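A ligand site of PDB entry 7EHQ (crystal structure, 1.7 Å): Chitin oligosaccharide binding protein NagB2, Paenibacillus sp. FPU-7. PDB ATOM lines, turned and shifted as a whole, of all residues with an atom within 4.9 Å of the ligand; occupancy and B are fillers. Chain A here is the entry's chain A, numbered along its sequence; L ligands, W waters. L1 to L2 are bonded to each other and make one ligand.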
ATOM      1  N   ILE A  37      22.370  20.772  14.731  1.00  0.00           N
ATOM      2  CA  ILE A  37      23.727  21.082  15.168  1.00  0.00           C
ATOM      3  C   ILE A  37      23.783  21.366  16.661  1.00  0.00           C
ATOM      4  O   ILE A  37      24.709  22.001  17.131  1.00  0.00           O
ATOM      5  CB  ILE A  37      24.319  22.253  14.347  1.00  0.00           C
ATOM      6  CG1 ILE A  37      23.442  23.508  14.450  1.00  0.00           C
ATOM      7  CG2 ILE A  37      24.461  21.836  12.888  1.00  0.00           C
ATOM      8  CD1 ILE A  37      24.172  24.823  13.960  1.00  0.00           C
ATOM      9  N   ASN A  38      22.813  20.853  17.421  1.00  0.00           N
ATOM     10  CA  ASN A  38      22.741  21.113  18.864  1.00  0.00           C
ATOM     11  C   ASN A  38      23.444  20.003  19.645  1.00  0.00           C
ATOM     12  O   ASN A  38      22.848  19.330  20.465  1.00  0.00           O
ATOM     13  CB  ASN A  38      21.290  21.231  19.306  1.00  0.00           C
ATOM     14  CG  ASN A  38      20.567  22.369  18.582  1.00  0.00           C
ATOM     15  OD1 ASN A  38      21.169  23.420  18.344  1.00  0.00           O
ATOM     16  ND2 ASN A  38      19.335  22.155  18.232  1.00  0.00           N
ATOM     17  N   ARG A  40      26.749  20.323  21.278  1.00  0.00           N
ATOM     18  CA  ARG A  40      27.618  20.689  22.391  1.00  0.00           C
ATOM     19  C   ARG A  40      26.861  20.685  23.712  1.00  0.00           C
ATOM     20  O   ARG A  40      25.647  20.873  23.759  1.00  0.00           O
ATOM     21  CB  ARG A  40      28.242  22.059  22.182  1.00  0.00           C
ATOM     22  CG  ARG A  40      29.214  22.139  21.019  1.00  0.00           C
ATOM     23  CD  ARG A  40      29.723  23.569  20.920  1.00  0.00           C
ATOM     24  NE  ARG A  40      30.566  23.775  19.754  1.00  0.00           N
ATOM     25  CZ  ARG A  40      30.294  24.626  18.766  1.00  0.00           C
ATOM     26  NH1 ARG A  40      29.188  25.354  18.816  1.00  0.00           N
ATOM     27  NH2 ARG A  40      31.120  24.746  17.755  1.00  0.00           N
ATOM     28  N   ASP A  73      28.668  22.044  14.038  1.00  0.00           N
ATOM     29  CA  ASP A  73      28.245  23.155  13.167  1.00  0.00           C
ATOM     30  C   ASP A  73      29.066  23.249  11.873  1.00  0.00           C
ATOM     31  O   ASP A  73      28.516  23.272  10.746  1.00  0.00           O
ATOM     32  CB  ASP A  73      28.264  24.504  13.918  1.00  0.00           C
ATOM     33  CG  ASP A  73      29.590  24.820  14.597  1.00  0.00           C
ATOM     34  OD1 ASP A  73      30.615  24.148  14.402  1.00  0.00           O
ATOM     35  OD2 ASP A  73      29.581  25.788  15.421  1.00  0.00           O
ATOM     36  N   THR A  74      30.404  23.316  11.990  1.00  0.00           N
ATOM     37  CA  THR A  74      31.170  23.465  10.777  1.00  0.00           C
ATOM     38  C   THR A  74      31.000  22.237   9.884  1.00  0.00           C
ATOM     39  O   THR A  74      30.849  22.362   8.680  1.00  0.00           O
ATOM     40  CB  THR A  74      32.666  23.691  11.092  1.00  0.00           C
ATOM     41  OG1 THR A  74      33.151  22.602  11.878  1.00  0.00           O
ATOM     42  CG2 THR A  74      32.865  25.034  11.843  1.00  0.00           C
ATOM     43  N   ARG A  77      27.496  22.212   7.942  1.00  0.00           N
ATOM     44  CA  ARG A  77      27.274  23.243   6.936  1.00  0.00           C
ATOM     45  C   ARG A  77      28.262  23.143   5.794  1.00  0.00           C
ATOM     46  O   ARG A  77      27.897  23.352   4.625  1.00  0.00           O
ATOM     47  CB  ARG A  77      27.370  24.636   7.587  1.00  0.00           C
ATOM     48  CG  ARG A  77      27.003  25.790   6.655  1.00  0.00           C
ATOM     49  CD  ARG A  77      27.326  27.161   7.250  1.00  0.00           C
ATOM     50  NE  ARG A  77      26.860  28.253   6.373  1.00  0.00           N
ATOM     51  CZ  ARG A  77      26.951  29.549   6.666  1.00  0.00           C
ATOM     52  NH1 ARG A  77      27.428  29.955   7.847  1.00  0.00           N
ATOM     53  NH2 ARG A  77      26.452  30.439   5.831  1.00  0.00           N
ATOM     54  N   PHE A  97      21.329  27.439   6.506  1.00  0.00           N
ATOM     55  CA  PHE A  97      21.648  28.877   6.587  1.00  0.00           C
ATOM     56  C   PHE A  97      21.027  29.636   5.434  1.00  0.00           C
ATOM     57  O   PHE A  97      21.035  29.167   4.295  1.00  0.00           O
ATOM     58  CB  PHE A  97      23.177  29.091   6.579  1.00  0.00           C
ATOM     59  CG  PHE A  97      23.755  29.018   7.964  1.00  0.00           C
ATOM     60  CD1 PHE A  97      24.154  27.795   8.478  1.00  0.00           C
ATOM     61  CD2 PHE A  97      23.798  30.144   8.761  1.00  0.00           C
ATOM     62  CE1 PHE A  97      24.650  27.681   9.757  1.00  0.00           C
ATOM     63  CE2 PHE A  97      24.316  30.069  10.035  1.00  0.00           C
ATOM     64  CZ  PHE A  97      24.735  28.820  10.551  1.00  0.00           C
ATOM     65  N   GLU A 144      15.056  29.632  12.950  1.00  0.00           N
ATOM     66  CA  GLU A 144      14.681  29.152  14.274  1.00  0.00           C
ATOM     67  C   GLU A 144      14.659  30.280  15.297  1.00  0.00           C
ATOM     68  O   GLU A 144      13.900  30.219  16.295  1.00  0.00           O
ATOM     69  CB  GLU A 144      15.691  28.075  14.673  1.00  0.00           C
ATOM     70  CG  GLU A 144      15.744  27.688  16.101  1.00  0.00           C
ATOM     71  CD  GLU A 144      16.914  26.746  16.388  1.00  0.00           C
ATOM     72  OE1 GLU A 144      17.343  26.024  15.471  1.00  0.00           O
ATOM     73  OE2 GLU A 144      17.404  26.760  17.511  1.00  0.00           O
ATOM     74  N   ALA A 145      15.490  31.297  15.083  1.00  0.00           N
ATOM     75  CA  ALA A 145      15.772  32.364  16.029  1.00  0.00           C
ATOM     76  C   ALA A 145      16.451  33.471  15.237  1.00  0.00           C
ATOM     77  O   ALA A 145      16.849  33.284  14.082  1.00  0.00           O
ATOM     78  CB  ALA A 145      16.685  31.888  17.193  1.00  0.00           C
ATOM     79  N   GLY A 146      16.618  34.624  15.877  1.00  0.00           N
ATOM     80  CA  GLY A 146      17.459  35.673  15.339  1.00  0.00           C
ATOM     81  C   GLY A 146      18.839  35.610  15.958  1.00  0.00           C
ATOM     82  O   GLY A 146      19.111  34.807  16.842  1.00  0.00           O
ATOM     83  N   PHE A 147      19.718  36.458  15.450  1.00  0.00           N
ATOM     84  CA  PHE A 147      21.005  36.623  16.102  1.00  0.00           C
ATOM     85  C   PHE A 147      21.416  38.094  16.027  1.00  0.00           C
ATOM     86  O   PHE A 147      20.968  38.843  15.143  1.00  0.00           O
ATOM     87  CB  PHE A 147      22.086  35.700  15.473  1.00  0.00           C
ATOM     88  CG  PHE A 147      22.697  36.248  14.238  1.00  0.00           C
ATOM     89  CD1 PHE A 147      22.061  36.084  12.994  1.00  0.00           C
ATOM     90  CD2 PHE A 147      23.905  36.926  14.299  1.00  0.00           C
ATOM     91  CE1 PHE A 147      22.602  36.637  11.838  1.00  0.00           C
ATOM     92  CE2 PHE A 147      24.463  37.479  13.177  1.00  0.00           C
ATOM     93  CZ  PHE A 147      23.829  37.312  11.911  1.00  0.00           C
ATOM     94  N   GLU A 149      25.575  39.917  16.907  1.00  0.00           N
ATOM     95  CA  GLU A 149      26.939  39.661  17.389  1.00  0.00           C
ATOM     96  C   GLU A 149      27.437  40.924  18.089  1.00  0.00           C
ATOM     97  O   GLU A 149      27.055  42.051  17.708  1.00  0.00           O
ATOM     98  CB  GLU A 149      27.881  39.253  16.250  1.00  0.00           C
ATOM     99  CG  GLU A 149      27.471  37.928  15.638  1.00  0.00           C
ATOM    100  CD  GLU A 149      28.388  37.411  14.575  1.00  0.00           C
ATOM    101  OE1 GLU A 149      29.510  37.954  14.364  1.00  0.00           O
ATOM    102  OE2 GLU A 149      27.978  36.423  13.922  1.00  0.00           O
ATOM    103  N   TRP A 198      35.867  30.568  11.329  1.00  0.00           N
ATOM    104  CA  TRP A 198      34.677  31.421  11.321  1.00  0.00           C
ATOM    105  C   TRP A 198      34.561  32.243  12.607  1.00  0.00           C
ATOM    106  O   TRP A 198      33.941  33.314  12.599  1.00  0.00           O
ATOM    107  CB  TRP A 198      33.398  30.555  11.117  1.00  0.00           C
ATOM    108  CG  TRP A 198      32.932  29.820  12.344  1.00  0.00           C
ATOM    109  CD1 TRP A 198      33.381  28.623  12.786  1.00  0.00           C
ATOM    110  CD2 TRP A 198      31.998  30.290  13.309  1.00  0.00           C
ATOM    111  NE1 TRP A 198      32.762  28.283  13.969  1.00  0.00           N
ATOM    112  CE2 TRP A 198      31.907  29.294  14.314  1.00  0.00           C
ATOM    113  CE3 TRP A 198      31.229  31.432  13.434  1.00  0.00           C
ATOM    114  CZ2 TRP A 198      31.071  29.430  15.411  1.00  0.00           C
ATOM    115  CZ3 TRP A 198      30.410  31.572  14.513  1.00  0.00           C
ATOM    116  CH2 TRP A 198      30.325  30.555  15.495  1.00  0.00           C
ATOM    117  N   TYR A 257      36.688  27.046  19.076  1.00  0.00           N
ATOM    118  CA  TYR A 257      35.649  28.051  19.344  1.00  0.00           C
ATOM    119  C   TYR A 257      35.151  27.993  20.783  1.00  0.00           C
ATOM    120  O   TYR A 257      35.182  28.987  21.524  1.00  0.00           O
ATOM    121  CB  TYR A 257      34.491  27.819  18.379  1.00  0.00           C
ATOM    122  CG  TYR A 257      33.272  28.661  18.612  1.00  0.00           C
ATOM    123  CD1 TYR A 257      33.346  30.059  18.612  1.00  0.00           C
ATOM    124  CD2 TYR A 257      32.024  28.055  18.835  1.00  0.00           C
ATOM    125  CE1 TYR A 257      32.197  30.840  18.789  1.00  0.00           C
ATOM    126  CE2 TYR A 257      30.892  28.822  19.008  1.00  0.00           C
ATOM    127  CZ  TYR A 257      30.987  30.212  18.997  1.00  0.00           C
ATOM    128  OH  TYR A 257      29.836  30.950  19.191  1.00  0.00           O
ATOM    129  N   TRP A 277      23.565  33.441  20.327  1.00  0.00           N
ATOM    130  CA  TRP A 277      23.433  32.023  20.699  1.00  0.00           C
ATOM    131  C   TRP A 277      24.397  31.638  21.785  1.00  0.00           C
ATOM    132  O   TRP A 277      24.280  30.514  22.335  1.00  0.00           O
ATOM    133  CB  TRP A 277      23.700  31.131  19.509  1.00  0.00           C
ATOM    134  CG  TRP A 277      25.048  31.376  18.857  1.00  0.00           C
ATOM    135  CD1 TRP A 277      26.261  30.843  19.254  1.00  0.00           C
ATOM    136  CD2 TRP A 277      25.323  32.228  17.750  1.00  0.00           C
ATOM    137  NE1 TRP A 277      27.280  31.330  18.408  1.00  0.00           N
ATOM    138  CE2 TRP A 277      26.708  32.184  17.499  1.00  0.00           C
ATOM    139  CE3 TRP A 277      24.519  33.047  16.947  1.00  0.00           C
ATOM    140  CZ2 TRP A 277      27.293  32.888  16.467  1.00  0.00           C
ATOM    141  CZ3 TRP A 277      25.132  33.761  15.916  1.00  0.00           C
ATOM    142  CH2 TRP A 277      26.517  33.686  15.698  1.00  0.00           C
ATOM    143  N   SER A 315      19.077  34.200  10.157  1.00  0.00           N
ATOM    144  CA  SER A 315      19.926  33.522   9.197  1.00  0.00           C
ATOM    145  C   SER A 315      19.952  32.009   9.318  1.00  0.00           C
ATOM    146  O   SER A 315      20.384  31.348   8.373  1.00  0.00           O
ATOM    147  CB  SER A 315      21.382  34.011   9.357  1.00  0.00           C
ATOM    148  OG  SER A 315      21.772  33.710  10.689  1.00  0.00           O
ATOM    149  N   ASN A 316      19.477  31.440  10.438  1.00  0.00           N
ATOM    150  CA  ASN A 316      19.743  30.044  10.700  1.00  0.00           C
ATOM    151  C   ASN A 316      18.463  29.393  11.211  1.00  0.00           C
ATOM    152  O   ASN A 316      17.819  29.938  12.119  1.00  0.00           O
ATOM    153  CB  ASN A 316      20.858  29.854  11.707  1.00  0.00           C
ATOM    154  CG  ASN A 316      21.238  28.378  11.871  1.00  0.00           C
ATOM    155  OD1 ASN A 316      21.185  27.827  12.989  1.00  0.00           O
ATOM    156  ND2 ASN A 316      21.598  27.736  10.756  1.00  0.00           N
ATOM    157  N   ARG A 354      17.675  32.859  23.267  1.00  0.00           N
ATOM    158  CA  ARG A 354      17.677  32.876  21.809  1.00  0.00           C
ATOM    159  C   ARG A 354      16.639  33.863  21.304  1.00  0.00           C
ATOM    160  O   ARG A 354      15.436  33.707  21.563  1.00  0.00           O
ATOM    161  CB  ARG A 354      17.511  31.452  21.262  1.00  0.00           C
ATOM    162  CG  ARG A 354      18.900  30.762  21.266  1.00  0.00           C
ATOM    163  CD  ARG A 354      18.861  29.274  21.140  1.00  0.00           C
ATOM    164  NE  ARG A 354      18.889  28.742  19.785  1.00  0.00           N
ATOM    165  CZ  ARG A 354      19.991  28.326  19.169  1.00  0.00           C
ATOM    166  NH1 ARG A 354      21.152  28.404  19.764  1.00  0.00           N
ATOM    167  NH2 ARG A 354      19.902  27.799  17.962  1.00  0.00           N
ATOM    168  N   ALA A 387      25.565  38.627   8.364  1.00  0.00           N
ATOM    169  CA  ALA A 387      26.916  38.082   8.302  1.00  0.00           C
ATOM    170  C   ALA A 387      27.374  37.951   6.861  1.00  0.00           C
ATOM    171  O   ALA A 387      26.579  37.629   5.962  1.00  0.00           O
ATOM    172  CB  ALA A 387      26.944  36.704   8.961  1.00  0.00           C
ATOM    173  N   ASP A 389      28.765  35.650   5.354  1.00  0.00           N
ATOM    174  CA  ASP A 389      28.550  34.365   4.723  1.00  0.00           C
ATOM    175  C   ASP A 389      27.123  34.183   4.225  1.00  0.00           C
ATOM    176  O   ASP A 389      26.838  33.197   3.516  1.00  0.00           O
ATOM    177  CB  ASP A 389      28.920  33.251   5.749  1.00  0.00           C
ATOM    178  CG  ASP A 389      28.214  33.441   7.032  1.00  0.00           C
ATOM    179  OD1 ASP A 389      28.743  34.204   7.887  1.00  0.00           O
ATOM    180  OD2 ASP A 389      27.082  32.882   7.195  1.00  0.00           O
HETATM  181  C1  LIG L   1      23.812  28.132  16.277  1.00  0.00           C
HETATM  182  C2  LIG L   1      23.258  29.394  15.604  1.00  0.00           C
HETATM  183  C3  LIG L   1      24.062  29.665  14.341  1.00  0.00           C
HETATM  184  C4  LIG L   1      25.567  29.704  14.644  1.00  0.00           C
HETATM  185  C5  LIG L   1      25.960  28.451  15.469  1.00  0.00           C
HETATM  186  C6  LIG L   1      27.389  28.477  15.949  1.00  0.00           C
HETATM  187  C7  LIG L   1      20.931  30.072  15.869  1.00  0.00           C
HETATM  188  C8  LIG L   1      19.519  29.885  15.396  1.00  0.00           C
HETATM  189  N1  LIG L   1      21.850  29.295  15.289  1.00  0.00           N
HETATM  190  O1  LIG L   1      23.073  27.721  17.357  1.00  0.00           O
HETATM  191  O2  LIG L   1      23.648  30.911  13.790  1.00  0.00           O
HETATM  192  O3  LIG L   1      26.286  29.588  13.432  1.00  0.00           O
HETATM  193  O4  LIG L   1      25.165  28.364  16.645  1.00  0.00           O
HETATM  194  O5  LIG L   1      27.642  27.242  16.601  1.00  0.00           O
HETATM  195  O6  LIG L   1      21.233  30.902  16.725  1.00  0.00           O
HETATM  196  C1  LG2 L   2      26.906  30.780  13.002  1.00  0.00           C
HETATM  197  C2  LG2 L   2      27.741  30.401  11.788  1.00  0.00           C
HETATM  198  C3  LG2 L   2      28.366  31.638  11.159  1.00  0.00           C
HETATM  199  C4  LG2 L   2      27.261  32.638  10.800  1.00  0.00           C
HETATM  200  C5  LG2 L   2      26.472  32.968  12.064  1.00  0.00           C
HETATM  201  C6  LG2 L   2      25.319  33.916  11.820  1.00  0.00           C
HETATM  202  C7  LG2 L   2      28.829  28.221  11.658  1.00  0.00           C
HETATM  203  C8  LG2 L   2      29.956  27.338  12.153  1.00  0.00           C
HETATM  204  N1  LG2 L   2      28.767  29.444  12.190  1.00  0.00           N
HETATM  205  O1  LG2 L   2      29.044  31.268   9.950  1.00  0.00           O
HETATM  206  O2  LG2 L   2      27.866  33.836  10.345  1.00  0.00           O
HETATM  207  O3  LG2 L   2      25.904  31.759  12.593  1.00  0.00           O
HETATM  208  O4  LG2 L   2      24.385  33.366  10.910  1.00  0.00           O
HETATM  209  O5  LG2 L   2      27.990  27.825  10.849  1.00  0.00           O
HETATM  210  O   HOH W   1      21.564  32.765  13.946  1.00  0.00           O
HETATM  211  O   HOH W   2      30.164  28.893   8.822  1.00  0.00           O
HETATM  212  O   HOH W   3      19.896  32.836  18.392  1.00  0.00           O
HETATM  213  O   HOH W   4      30.975  32.965   8.992  1.00  0.00           O
HETATM  214  O   HOH W   5      25.878  25.104  17.160  1.00  0.00           O
HETATM  215  O   HOH W   6      23.310  25.433  18.101  1.00  0.00           O
HETATM  216  O   HOH W   7      26.319  27.544  19.386  1.00  0.00           O
HETATM  217  O   HOH W   8      29.479  35.632  11.866  1.00  0.00           O
HETATM  218  O   HOH W   9      24.933  33.958   8.329  1.00  0.00           O
HETATM  219  O   HOH W  10      26.642  25.259  11.000  1.00  0.00           O
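Residues that only touch the ligand: Thr 74, Phe 97, Ala 145, Phe 147, Trp 198, Trp 277 and Ala 387.
Hydrophobic or aromatic side chains that line the ligand: Phe 97, Ala 145, Phe 147, Trp 198, Trp 277 and Ala 387.
Of the 20 residues printed, 14 come within 4 Å of the ligand.
The nearest printed residue that does not touch the ligand is Ile 37 (4.1 Å).
The guanidinium group (NH2) of Arg 77 lies within salt-bridge range of the side-chain carboxylate (OD2) of Asp 389, at 2.9 Å.
The backbone carbonyl oxygen (O) of Asn 316 is in hydrogen-bond range of the backbone NH (N) of Glu 144, 2.9 Å away.
The guanidinium group (NH2) of Arg 354 is in salt-bridge range of the side-chain carboxylate (OE2) of Glu 144.
The side-chain hydroxyl (OH) of Tyr 257 sits at hydrogen-bond distance from the indole nitrogen (NE1) of Trp 277 (2.7 Å).
The side-chain carboxylate (OD2) of Asp 73 is in salt-bridge range of the guanidinium group (NH2) of Arg 40 (3.0 Å).
Water W6 lies within hydrogen-bond range of an oxygen (O1) of LIG L1 (2.4 Å) and the side-chain amide oxygen (OD1) of Asn 38 (2.9 Å).
Water W9 lies within hydrogen-bond range of OD2 of Asp 389 (2.7 Å) and O4 of LG2 L2 (2.7 Å).
Water W4 lies within hydrogen-bond range of O1 of LG2 L2 (2.7 Å) and OD1 of Asp 389 (2.8 Å).
Water W5 lies within hydrogen-bond range of an oxygen (O5) of LIG L1 and the backbone carbonyl oxygen (O) of Ile 37.
Water W8 lies within hydrogen-bond range of OE2 of Glu 149 (2.7 Å) and O2 of LG2 L2 (2.9 Å).
Water W2 lies within hydrogen-bond range of an oxygen (O1) of LG2 L2 and the guanidinium group of Arg 77.
O1 of LG2 L2 lies within hydrogen-bond range of NH1 of Arg 77, at 3.0 Å.
The side-chain carboxylate (OD1) of Asp 389 is in hydrogen-bond range of an oxygen (O2) of LG2 L2 (2.6 Å).
The side-chain amide oxygen (OD1) of Asn 316 lies within hydrogen-bond range of a nitrogen (N1) of LIG L1 (2.8 Å).
The guanidinium group (NH1) of Arg 354 lies within hydrogen-bond range of an oxygen (O1) of LIG L1.
The side-chain hydroxyl of Ser 315 lies within hydrogen-bond range of an oxygen (O4) of LG2 L2 (2.6 Å).
NH1 of Arg 40 lies within hydrogen-bond range of O5 of LIG L1, 3.3 Å away.
OD2 of Asp 73 lies within hydrogen-bond range of O5 of LIG L1 (2.7 Å).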
